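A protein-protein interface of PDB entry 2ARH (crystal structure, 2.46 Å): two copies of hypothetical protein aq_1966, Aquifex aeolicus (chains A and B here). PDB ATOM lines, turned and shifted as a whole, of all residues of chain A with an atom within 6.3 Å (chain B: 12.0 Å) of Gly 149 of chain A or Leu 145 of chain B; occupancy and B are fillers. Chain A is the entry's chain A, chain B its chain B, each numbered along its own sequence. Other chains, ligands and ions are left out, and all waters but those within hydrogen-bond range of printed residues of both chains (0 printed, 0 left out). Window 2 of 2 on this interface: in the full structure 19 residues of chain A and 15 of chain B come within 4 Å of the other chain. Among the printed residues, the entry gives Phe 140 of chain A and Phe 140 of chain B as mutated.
Met 146 of chain A touches its own counterpart, Met 146 of chain B.
Of the 12 pairs that touch across the chains among the printed residues, 1 has its exchanged pair printed and touching as well.
The backbone NH (N) of Gly 148 of chain A is in hydrogen-bond range of the side-chain carboxylate (OE2) of Glu 143 of chain A, at 2.8 Å.
N of Phe 140 of chain A is in hydrogen-bond range of O of Gly 149 of chain A (3.3 Å).
The side-chain carboxylate (OE1) of Glu 143 of chain B is in hydrogen-bond range of the backbone NH (N) of Gly 148 of chain B, 2.8 Å away.
The side-chain amino group of Lys 151 of chain A sits close to the backbone carbonyl oxygen of Gly 148 of chain A, 3.1 Å away.
O of Trp 139 of chain A is in hydrogen-bond range of OH of Tyr 103 of chain A, 2.7 Å away.
N of Trp 139 of chain A lies within hydrogen-bond range of O of Lys 151 of chain A (2.8 Å).
Of the 13 printed residues of chain B, 5 touch a printed residue of chain A.
Hydrophobic or aromatic side chains of chain B that line the printed part of chain A: Pro 142, Leu 145 and Met 146.
Printed residues of chain A that touch a printed residue of chain B: Glu 67, Phe 100, Trp 139, Met 146, Gly 148, Gly 149, Lys 151 and Gln 153.
O of Leu 145 of chain B lies within hydrogen-bond range of NZ of Lys 151 of chain A (3.0 Å).
O of Gly 144 of chain B sits close to OE2 of Glu 67 of chain A (3.3 Å).
The side-chain amino group (NZ) of Lys 151 of chain A lies within hydrogen-bond range of the backbone carbonyl oxygen (O) of Gly 144 of chain B (2.7 Å).
O of Gly 148 of chain A sits close to O of Leu 145 of chain B, at 3.2 Å.
Phe 100 of chain A touches Pro 142 of chain B (CZ to CB, 3.9 Å).
Glu 143 of chain B touches Phe 100 of chain A (O to CZ, 3.5 Å).
CD2 of Phe 100 of chain A touches C of Gly 144 of chain B, 3.7 Å away.
Phe 100 of chain A touches Leu 145 of chain B.
CD2 of Leu 145 of chain B touches CG of Trp 139 of chain A (3.9 Å).
SD of Met 146 of chain A touches CG of Met 146 of chain B (3.7 Å).
Gly 149 of chain A touches Leu 145 of chain B.
Gln 153 of chain A touches Pro 142 of chain B.
Of the printed residues of chain B, Gly 149 of chain A touches Leu 145.
Of chain A, only Phe 100, Trp 139, Gly 148, Gly 149 and Lys 151 come within 4 Å of Leu 145 of chain B.
No residue of chain B comes within 4 Å of Ile 141 of chain A.
No residue of chain B comes within 4 Å of Pro 142 of chain A.
Of the printed residues of chain B, Met 146 of chain A touches Met 146 (3.7 Å).
Gly 148 of chain A touches just one residue of chain B: Leu 145.
His 150 of chain A touches none of the printed residues of chain B.
Lys 151 of chain A touches two residues of chain B.
Printed residues of chain B within 4 Å of Gln 153 of chain A: Pro 142 (3.9 Å).
Of the printed residues of chain B, Phe 100 of chain A touches Pro 142, Glu 143, Gly 144 and Leu 145.
Printed residues of chain A within 4 Å of Gly 144 of chain B: Glu 67 (3.2 Å), Phe 100 (3.7 Å) and Lys 151 (2.7 Å).
Of the printed residues of chain A, Glu 143 of chain B touches Phe 100.
Printed residues of chain A within 4 Å of Pro 142 of chain B: Phe 100 (3.9 Å) and Gln 153 (3.9 Å).
Glu 147 of chain A touches none of the printed residues of chain B.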
ATOM      1  N   GLU A  67      25.752  26.782   0.354  1.00  0.00           N
ATOM      2  CA  GLU A  67      24.372  26.424   0.146  1.00  0.00           C
ATOM      3  C   GLU A  67      23.505  27.531   0.705  1.00  0.00           C
ATOM      4  O   GLU A  67      23.536  27.772   1.902  1.00  0.00           O
ATOM      5  CB  GLU A  67      24.072  25.135   0.883  1.00  0.00           C
ATOM      6  CG  GLU A  67      22.699  24.628   0.597  1.00  0.00           C
ATOM      7  CD  GLU A  67      22.240  23.594   1.604  1.00  0.00           C
ATOM      8  OE1 GLU A  67      23.073  22.998   2.325  1.00  0.00           O
ATOM      9  OE2 GLU A  67      21.032  23.342   1.629  1.00  0.00           O
ATOM     10  N   PHE A 100      24.778  26.347  -4.247  1.00  0.00           N
ATOM     11  CA  PHE A 100      23.439  25.765  -4.234  1.00  0.00           C
ATOM     12  C   PHE A 100      22.493  26.849  -3.730  1.00  0.00           C
ATOM     13  O   PHE A 100      22.754  27.499  -2.682  1.00  0.00           O
ATOM     14  CB  PHE A 100      23.311  24.582  -3.280  1.00  0.00           C
ATOM     15  CG  PHE A 100      24.291  23.464  -3.522  1.00  0.00           C
ATOM     16  CD1 PHE A 100      25.624  23.565  -3.056  1.00  0.00           C
ATOM     17  CD2 PHE A 100      23.860  22.272  -4.142  1.00  0.00           C
ATOM     18  CE1 PHE A 100      26.514  22.563  -3.255  1.00  0.00           C
ATOM     19  CE2 PHE A 100      24.774  21.220  -4.346  1.00  0.00           C
ATOM     20  CZ  PHE A 100      26.113  21.392  -3.913  1.00  0.00           C
ATOM     21  N   GLU A 102      18.445  27.281  -2.876  1.00  0.00           N
ATOM     22  CA  GLU A 102      17.065  26.791  -2.773  1.00  0.00           C
ATOM     23  C   GLU A 102      16.070  27.728  -3.462  1.00  0.00           C
ATOM     24  O   GLU A 102      15.971  28.900  -3.089  1.00  0.00           O
ATOM     25  CB  GLU A 102      16.705  26.586  -1.313  1.00  0.00           C
ATOM     26  CG  GLU A 102      15.403  25.883  -1.145  1.00  0.00           C
ATOM     27  CD  GLU A 102      15.237  25.405   0.256  1.00  0.00           C
ATOM     28  OE1 GLU A 102      15.245  26.275   1.157  1.00  0.00           O
ATOM     29  OE2 GLU A 102      15.105  24.171   0.444  1.00  0.00           O
ATOM     30  N   TYR A 103      15.358  27.223  -4.473  1.00  0.00           N
ATOM     31  CA  TYR A 103      14.477  28.071  -5.281  1.00  0.00           C
ATOM     32  C   TYR A 103      12.974  27.946  -4.927  1.00  0.00           C
ATOM     33  O   TYR A 103      12.127  28.593  -5.580  1.00  0.00           O
ATOM     34  CB  TYR A 103      14.698  27.849  -6.800  1.00  0.00           C
ATOM     35  CG  TYR A 103      14.348  26.452  -7.327  1.00  0.00           C
ATOM     36  CD1 TYR A 103      13.019  26.056  -7.504  1.00  0.00           C
ATOM     37  CD2 TYR A 103      15.354  25.528  -7.622  1.00  0.00           C
ATOM     38  CE1 TYR A 103      12.687  24.747  -7.949  1.00  0.00           C
ATOM     39  CE2 TYR A 103      15.047  24.239  -8.089  1.00  0.00           C
ATOM     40  CZ  TYR A 103      13.706  23.860  -8.240  1.00  0.00           C
ATOM     41  OH  TYR A 103      13.402  22.608  -8.703  1.00  0.00           O
ATOM     42  N   ASP A 138      19.341  21.521 -12.058  1.00  0.00           N
ATOM     43  CA  ASP A 138      18.009  21.818 -11.484  1.00  0.00           C
ATOM     44  C   ASP A 138      17.591  20.590 -10.668  1.00  0.00           C
ATOM     45  O   ASP A 138      17.202  19.564 -11.242  1.00  0.00           O
ATOM     46  CB  ASP A 138      16.993  22.040 -12.652  1.00  0.00           C
ATOM     47  CG  ASP A 138      15.553  22.326 -12.185  1.00  0.00           C
ATOM     48  OD1 ASP A 138      15.330  22.742 -11.017  1.00  0.00           O
ATOM     49  OD2 ASP A 138      14.608  22.177 -12.993  1.00  0.00           O
ATOM     50  N   TRP A 139      17.654  20.665  -9.344  1.00  0.00           N
ATOM     51  CA  TRP A 139      17.162  19.569  -8.580  1.00  0.00           C
ATOM     52  C   TRP A 139      15.702  19.789  -8.311  1.00  0.00           C
ATOM     53  O   TRP A 139      15.302  20.890  -7.961  1.00  0.00           O
ATOM     54  CB  TRP A 139      17.912  19.383  -7.281  1.00  0.00           C
ATOM     55  CG  TRP A 139      19.358  19.009  -7.435  1.00  0.00           C
ATOM     56  CD1 TRP A 139      20.459  19.863  -7.424  1.00  0.00           C
ATOM     57  CD2 TRP A 139      19.888  17.679  -7.579  1.00  0.00           C
ATOM     58  NE1 TRP A 139      21.620  19.117  -7.515  1.00  0.00           N
ATOM     59  CE2 TRP A 139      21.304  17.793  -7.624  1.00  0.00           C
ATOM     60  CE3 TRP A 139      19.305  16.408  -7.651  1.00  0.00           C
ATOM     61  CZ2 TRP A 139      22.133  16.692  -7.752  1.00  0.00           C
ATOM     62  CZ3 TRP A 139      20.130  15.295  -7.772  1.00  0.00           C
ATOM     63  CH2 TRP A 139      21.534  15.435  -7.836  1.00  0.00           C
ATOM     64  N   PHE A 140      14.901  18.740  -8.467  1.00  0.00           N
ATOM     65  CA  PHE A 140      13.454  18.866  -8.215  1.00  0.00           C
ATOM     66  C   PHE A 140      12.884  17.640  -7.518  1.00  0.00           C
ATOM     67  O   PHE A 140      12.034  16.938  -8.064  1.00  0.00           O
ATOM     68  CB  PHE A 140      12.654  19.255  -9.485  1.00  0.00           C
ATOM     69  CG  PHE A 140      12.947  18.430 -10.693  1.00  0.00           C
ATOM     70  CD1 PHE A 140      13.932  18.812 -11.596  1.00  0.00           C
ATOM     71  CD2 PHE A 140      12.186  17.281 -10.987  1.00  0.00           C
ATOM     72  CE1 PHE A 140      14.183  18.053 -12.774  1.00  0.00           C
ATOM     73  CE2 PHE A 140      12.445  16.501 -12.163  1.00  0.00           C
ATOM     74  CZ  PHE A 140      13.453  16.905 -13.059  1.00  0.00           C
ATOM     75  N   ILE A 141      13.388  17.390  -6.311  1.00  0.00           N
ATOM     76  CA  ILE A 141      13.076  16.171  -5.571  1.00  0.00           C
ATOM     77  C   ILE A 141      11.919  16.433  -4.647  1.00  0.00           C
ATOM     78  O   ILE A 141      11.948  17.401  -3.905  1.00  0.00           O
ATOM     79  CB  ILE A 141      14.295  15.660  -4.750  1.00  0.00           C
ATOM     80  CG1 ILE A 141      15.354  15.077  -5.703  1.00  0.00           C
ATOM     81  CG2 ILE A 141      13.842  14.653  -3.632  1.00  0.00           C
ATOM     82  CD1 ILE A 141      16.726  14.769  -5.046  1.00  0.00           C
ATOM     83  N   PRO A 142      10.892  15.569  -4.676  1.00  0.00           N
ATOM     84  CA  PRO A 142       9.710  15.954  -3.890  1.00  0.00           C
ATOM     85  C   PRO A 142       9.967  16.076  -2.361  1.00  0.00           C
ATOM     86  O   PRO A 142      10.528  15.183  -1.722  1.00  0.00           O
ATOM     87  CB  PRO A 142       8.691  14.867  -4.218  1.00  0.00           C
ATOM     88  CG  PRO A 142       9.252  14.094  -5.372  1.00  0.00           C
ATOM     89  CD  PRO A 142      10.726  14.264  -5.352  1.00  0.00           C
ATOM     90  N   GLU A 143       9.533  17.201  -1.806  1.00  0.00           N
ATOM     91  CA  GLU A 143       9.660  17.545  -0.408  1.00  0.00           C
ATOM     92  C   GLU A 143       9.023  16.536   0.578  1.00  0.00           C
ATOM     93  O   GLU A 143       9.361  16.525   1.794  1.00  0.00           O
ATOM     94  CB  GLU A 143       9.082  18.946  -0.226  1.00  0.00           C
ATOM     95  CG  GLU A 143       9.885  19.823   0.746  1.00  0.00           C
ATOM     96  CD  GLU A 143      11.150  20.516   0.159  1.00  0.00           C
ATOM     97  OE1 GLU A 143      11.345  20.702  -1.081  1.00  0.00           O
ATOM     98  OE2 GLU A 143      11.967  20.898   1.006  1.00  0.00           O
ATOM     99  N   MET A 146      11.989  13.969   0.681  1.00  0.00           N
ATOM    100  CA  MET A 146      13.163  14.506   1.343  1.00  0.00           C
ATOM    101  C   MET A 146      13.042  16.038   1.281  1.00  0.00           C
ATOM    102  O   MET A 146      12.965  16.604   0.185  1.00  0.00           O
ATOM    103  CB  MET A 146      14.401  14.006   0.585  1.00  0.00           C
ATOM    104  CG  MET A 146      15.737  14.454   1.096  1.00  0.00           C
ATOM    105  SD  MET A 146      17.095  14.579  -0.360  1.00  0.00           S
ATOM    106  CE  MET A 146      16.434  13.151  -1.609  1.00  0.00           C
ATOM    107  N   GLU A 147      12.981  16.686   2.447  1.00  0.00           N
ATOM    108  CA  GLU A 147      13.152  18.147   2.549  1.00  0.00           C
ATOM    109  C   GLU A 147      14.487  18.571   1.861  1.00  0.00           C
ATOM    110  O   GLU A 147      15.443  17.797   1.840  1.00  0.00           O
ATOM    111  CB  GLU A 147      13.081  18.614   4.032  1.00  0.00           C
ATOM    112  CG  GLU A 147      11.640  18.452   4.711  1.00  0.00           C
ATOM    113  CD  GLU A 147      11.633  18.209   6.251  1.00  0.00           C
ATOM    114  OE1 GLU A 147      10.713  17.511   6.734  1.00  0.00           O
ATOM    115  OE2 GLU A 147      12.532  18.692   7.001  1.00  0.00           O
ATOM    116  N   GLY A 148      14.499  19.762   1.252  1.00  0.00           N
ATOM    117  CA  GLY A 148      15.689  20.338   0.654  1.00  0.00           C
ATOM    118  C   GLY A 148      16.107  19.879  -0.740  1.00  0.00           C
ATOM    119  O   GLY A 148      17.263  19.887  -1.041  1.00  0.00           O
ATOM    120  N   GLY A 149      15.177  19.511  -1.607  1.00  0.00           N
ATOM    121  CA  GLY A 149      15.536  19.006  -2.920  1.00  0.00           C
ATOM    122  C   GLY A 149      15.092  19.852  -4.097  1.00  0.00           C
ATOM    123  O   GLY A 149      15.096  19.380  -5.230  1.00  0.00           O
ATOM    124  N   HIS A 150      14.743  21.107  -3.839  1.00  0.00           N
ATOM    125  CA  HIS A 150      14.465  22.096  -4.890  1.00  0.00           C
ATOM    126  C   HIS A 150      15.534  23.162  -4.901  1.00  0.00           C
ATOM    127  O   HIS A 150      15.353  24.275  -4.429  1.00  0.00           O
ATOM    128  CB  HIS A 150      13.047  22.675  -4.767  1.00  0.00           C
ATOM    129  CG  HIS A 150      11.991  21.648  -5.026  1.00  0.00           C
ATOM    130  ND1 HIS A 150      11.401  20.912  -4.014  1.00  0.00           N
ATOM    131  CD2 HIS A 150      11.478  21.174  -6.187  1.00  0.00           C
ATOM    132  CE1 HIS A 150      10.531  20.066  -4.538  1.00  0.00           C
ATOM    133  NE2 HIS A 150      10.558  20.205  -5.853  1.00  0.00           N
ATOM    134  N   LYS A 151      16.662  22.786  -5.483  1.00  0.00           N
ATOM    135  CA  LYS A 151      17.861  23.605  -5.479  1.00  0.00           C
ATOM    136  C   LYS A 151      18.377  23.722  -6.869  1.00  0.00           C
ATOM    137  O   LYS A 151      18.236  22.780  -7.655  1.00  0.00           O
ATOM    138  CB  LYS A 151      18.906  22.952  -4.641  1.00  0.00           C
ATOM    139  CG  LYS A 151      18.803  23.293  -3.177  1.00  0.00           C
ATOM    140  CD  LYS A 151      19.444  22.214  -2.293  1.00  0.00           C
ATOM    141  CE  LYS A 151      18.917  22.317  -0.880  1.00  0.00           C
ATOM    142  NZ  LYS A 151      19.752  21.437   0.038  1.00  0.00           N
ATOM    143  N   GLN A 153      22.011  24.012  -8.517  1.00  0.00           N
ATOM    144  CA  GLN A 153      23.395  23.714  -8.224  1.00  0.00           C
ATOM    145  C   GLN A 153      24.207  24.252  -9.390  1.00  0.00           C
ATOM    146  O   GLN A 153      23.917  23.950 -10.536  1.00  0.00           O
ATOM    147  CB  GLN A 153      23.575  22.200  -8.062  1.00  0.00           C
ATOM    148  CG  GLN A 153      24.965  21.794  -7.669  1.00  0.00           C
ATOM    149  CD  GLN A 153      25.250  20.288  -7.872  1.00  0.00           C
ATOM    150  OE1 GLN A 153      24.409  19.436  -7.637  1.00  0.00           O
ATOM    151  NE2 GLN A 153      26.459  19.984  -8.301  1.00  0.00           N
ATOM    152  N   PHE B 104      33.736  10.722   4.252  1.00  0.00           N
ATOM    153  CA  PHE B 104      33.977  12.107   3.978  1.00  0.00           C
ATOM    154  C   PHE B 104      35.217  12.602   4.710  1.00  0.00           C
ATOM    155  O   PHE B 104      36.026  13.345   4.162  1.00  0.00           O
ATOM    156  CB  PHE B 104      32.731  12.941   4.354  1.00  0.00           C
ATOM    157  CG  PHE B 104      32.776  14.383   3.838  1.00  0.00           C
ATOM    158  CD1 PHE B 104      32.048  14.749   2.710  1.00  0.00           C
ATOM    159  CD2 PHE B 104      33.595  15.364   4.468  1.00  0.00           C
ATOM    160  CE1 PHE B 104      32.084  16.060   2.202  1.00  0.00           C
ATOM    161  CE2 PHE B 104      33.629  16.687   3.993  1.00  0.00           C
ATOM    162  CZ  PHE B 104      32.853  17.035   2.862  1.00  0.00           C
ATOM    163  N   TRP B 139      28.341   5.832  -2.745  1.00  0.00           N
ATOM    164  CA  TRP B 139      27.440   6.941  -2.820  1.00  0.00           C
ATOM    165  C   TRP B 139      28.253   8.228  -2.745  1.00  0.00           C
ATOM    166  O   TRP B 139      29.085   8.429  -1.842  1.00  0.00           O
ATOM    167  CB  TRP B 139      26.479   6.919  -1.664  1.00  0.00           C
ATOM    168  CG  TRP B 139      25.631   5.738  -1.566  1.00  0.00           C
ATOM    169  CD1 TRP B 139      25.888   4.570  -0.848  1.00  0.00           C
ATOM    170  CD2 TRP B 139      24.333   5.583  -2.140  1.00  0.00           C
ATOM    171  NE1 TRP B 139      24.814   3.719  -0.950  1.00  0.00           N
ATOM    172  CE2 TRP B 139      23.846   4.306  -1.733  1.00  0.00           C
ATOM    173  CE3 TRP B 139      23.524   6.397  -2.960  1.00  0.00           C
ATOM    174  CZ2 TRP B 139      22.577   3.821  -2.126  1.00  0.00           C
ATOM    175  CZ3 TRP B 139      22.265   5.919  -3.344  1.00  0.00           C
ATOM    176  CH2 TRP B 139      21.798   4.634  -2.908  1.00  0.00           C
ATOM    177  N   PHE B 140      28.002   9.096  -3.708  1.00  0.00           N
ATOM    178  CA  PHE B 140      28.642  10.376  -3.747  1.00  0.00           C
ATOM    179  C   PHE B 140      27.596  11.396  -4.097  1.00  0.00           C
ATOM    180  O   PHE B 140      27.541  11.852  -5.222  1.00  0.00           O
ATOM    181  CB  PHE B 140      29.897  10.413  -4.674  1.00  0.00           C
ATOM    182  CG  PHE B 140      29.788   9.593  -5.922  1.00  0.00           C
ATOM    183  CD1 PHE B 140      29.417  10.178  -7.130  1.00  0.00           C
ATOM    184  CD2 PHE B 140      30.139   8.256  -5.928  1.00  0.00           C
ATOM    185  CE1 PHE B 140      29.352   9.430  -8.308  1.00  0.00           C
ATOM    186  CE2 PHE B 140      30.080   7.488  -7.097  1.00  0.00           C
ATOM    187  CZ  PHE B 140      29.687   8.081  -8.292  1.00  0.00           C
ATOM    188  N   ILE B 141      26.746  11.733  -3.136  1.00  0.00           N
ATOM    189  CA  ILE B 141      25.773  12.774  -3.388  1.00  0.00           C
ATOM    190  C   ILE B 141      26.217  14.139  -2.797  1.00  0.00           C
ATOM    191  O   ILE B 141      26.827  14.187  -1.760  1.00  0.00           O
ATOM    192  CB  ILE B 141      24.198  12.358  -3.204  1.00  0.00           C
ATOM    193  CG1 ILE B 141      23.412  13.336  -2.352  1.00  0.00           C
ATOM    194  CG2 ILE B 141      23.876  10.835  -2.874  1.00  0.00           C
ATOM    195  CD1 ILE B 141      22.209  13.730  -3.066  1.00  0.00           C
ATOM    196  N   PRO B 142      25.972  15.250  -3.510  1.00  0.00           N
ATOM    197  CA  PRO B 142      26.507  16.496  -2.975  1.00  0.00           C
ATOM    198  C   PRO B 142      25.914  16.839  -1.598  1.00  0.00           C
ATOM    199  O   PRO B 142      24.694  16.778  -1.414  1.00  0.00           O
ATOM    200  CB  PRO B 142      26.126  17.538  -4.053  1.00  0.00           C
ATOM    201  CG  PRO B 142      25.923  16.736  -5.308  1.00  0.00           C
ATOM    202  CD  PRO B 142      25.325  15.431  -4.830  1.00  0.00           C
ATOM    203  N   GLU B 143      26.779  17.131  -0.610  1.00  0.00           N
ATOM    204  CA  GLU B 143      26.290  17.746   0.627  1.00  0.00           C
ATOM    205  C   GLU B 143      25.900  19.104   0.008  1.00  0.00           C
ATOM    206  O   GLU B 143      26.483  19.522  -1.001  1.00  0.00           O
ATOM    207  CB  GLU B 143      27.400  17.927   1.663  1.00  0.00           C
ATOM    208  CG  GLU B 143      28.365  16.782   1.850  1.00  0.00           C
ATOM    209  CD  GLU B 143      27.879  15.661   2.772  1.00  0.00           C
ATOM    210  OE1 GLU B 143      26.967  15.865   3.627  1.00  0.00           O
ATOM    211  OE2 GLU B 143      28.430  14.548   2.621  1.00  0.00           O
ATOM    212  N   GLY B 144      24.937  19.817   0.467  1.00  0.00           N
ATOM    213  CA  GLY B 144      24.603  20.917  -0.438  1.00  0.00           C
ATOM    214  C   GLY B 144      23.219  20.626  -0.933  1.00  0.00           C
ATOM    215  O   GLY B 144      22.317  21.439  -0.760  1.00  0.00           O
ATOM    216  N   LEU B 145      23.051  19.441  -1.508  1.00  0.00           N
ATOM    217  CA  LEU B 145      21.751  18.871  -1.810  1.00  0.00           C
ATOM    218  C   LEU B 145      21.126  18.135  -0.601  1.00  0.00           C
ATOM    219  O   LEU B 145      19.957  18.421  -0.179  1.00  0.00           O
ATOM    220  CB  LEU B 145      21.827  17.976  -3.059  1.00  0.00           C
ATOM    221  CG  LEU B 145      20.519  17.438  -3.709  1.00  0.00           C
ATOM    222  CD1 LEU B 145      20.205  16.049  -3.260  1.00  0.00           C
ATOM    223  CD2 LEU B 145      19.287  18.365  -3.562  1.00  0.00           C
ATOM    224  N   MET B 146      21.914  17.219  -0.030  1.00  0.00           N
ATOM    225  CA  MET B 146      21.472  16.347   1.037  1.00  0.00           C
ATOM    226  C   MET B 146      22.720  15.959   1.796  1.00  0.00           C
ATOM    227  O   MET B 146      23.660  15.400   1.226  1.00  0.00           O
ATOM    228  CB  MET B 146      20.799  15.100   0.436  1.00  0.00           C
ATOM    229  CG  MET B 146      20.248  14.064   1.422  1.00  0.00           C
ATOM    230  SD  MET B 146      20.313  12.206   0.613  1.00  0.00           S
ATOM    231  CE  MET B 146      22.226  11.834   1.159  1.00  0.00           C
ATOM    232  N   GLU B 147      22.732  16.276   3.084  1.00  0.00           N
ATOM    233  CA  GLU B 147      23.859  15.940   3.949  1.00  0.00           C
ATOM    234  C   GLU B 147      23.927  14.424   4.160  1.00  0.00           C
ATOM    235  O   GLU B 147      22.917  13.741   4.082  1.00  0.00           O
ATOM    236  CB  GLU B 147      23.717  16.656   5.296  1.00  0.00           C
ATOM    237  CG  GLU B 147      24.003  18.161   5.277  1.00  0.00           C
ATOM    238  CD  GLU B 147      24.148  18.727   6.708  1.00  0.00           C
ATOM    239  OE1 GLU B 147      25.132  18.347   7.424  1.00  0.00           O
ATOM    240  OE2 GLU B 147      23.269  19.532   7.113  1.00  0.00           O
ATOM    241  N   GLY B 148      25.115  13.897   4.400  1.00  0.00           N
ATOM    242  CA  GLY B 148      25.243  12.467   4.673  1.00  0.00           C
ATOM    243  C   GLY B 148      25.238  11.530   3.484  1.00  0.00           C
ATOM    244  O   GLY B 148      25.004  10.351   3.645  1.00  0.00           O
ATOM    245  N   GLY B 149      25.536  12.022   2.293  1.00  0.00           N
ATOM    246  CA  GLY B 149      25.582  11.141   1.117  1.00  0.00           C
ATOM    247  C   GLY B 149      26.922  10.760   0.503  1.00  0.00           C
ATOM    248  O   GLY B 149      26.964  10.452  -0.672  1.00  0.00           O
ATOM    249  N   HIS B 150      27.999  10.787   1.294  1.00  0.00           N
ATOM    250  CA  HIS B 150      29.339  10.227   0.924  1.00  0.00           C
ATOM    251  C   HIS B 150      29.684   9.002   1.768  1.00  0.00           C
ATOM    252  O   HIS B 150      30.457   9.081   2.737  1.00  0.00           O
ATOM    253  CB  HIS B 150      30.455  11.294   1.000  1.00  0.00           C
ATOM    254  CG  HIS B 150      30.226  12.428   0.055  1.00  0.00           C
ATOM    255  ND1 HIS B 150      30.527  12.342  -1.293  1.00  0.00           N
ATOM    256  CD2 HIS B 150      29.595  13.611   0.230  1.00  0.00           C
ATOM    257  CE1 HIS B 150      30.139  13.457  -1.889  1.00  0.00           C
ATOM    258  NE2 HIS B 150      29.568  14.240  -0.987  1.00  0.00           N
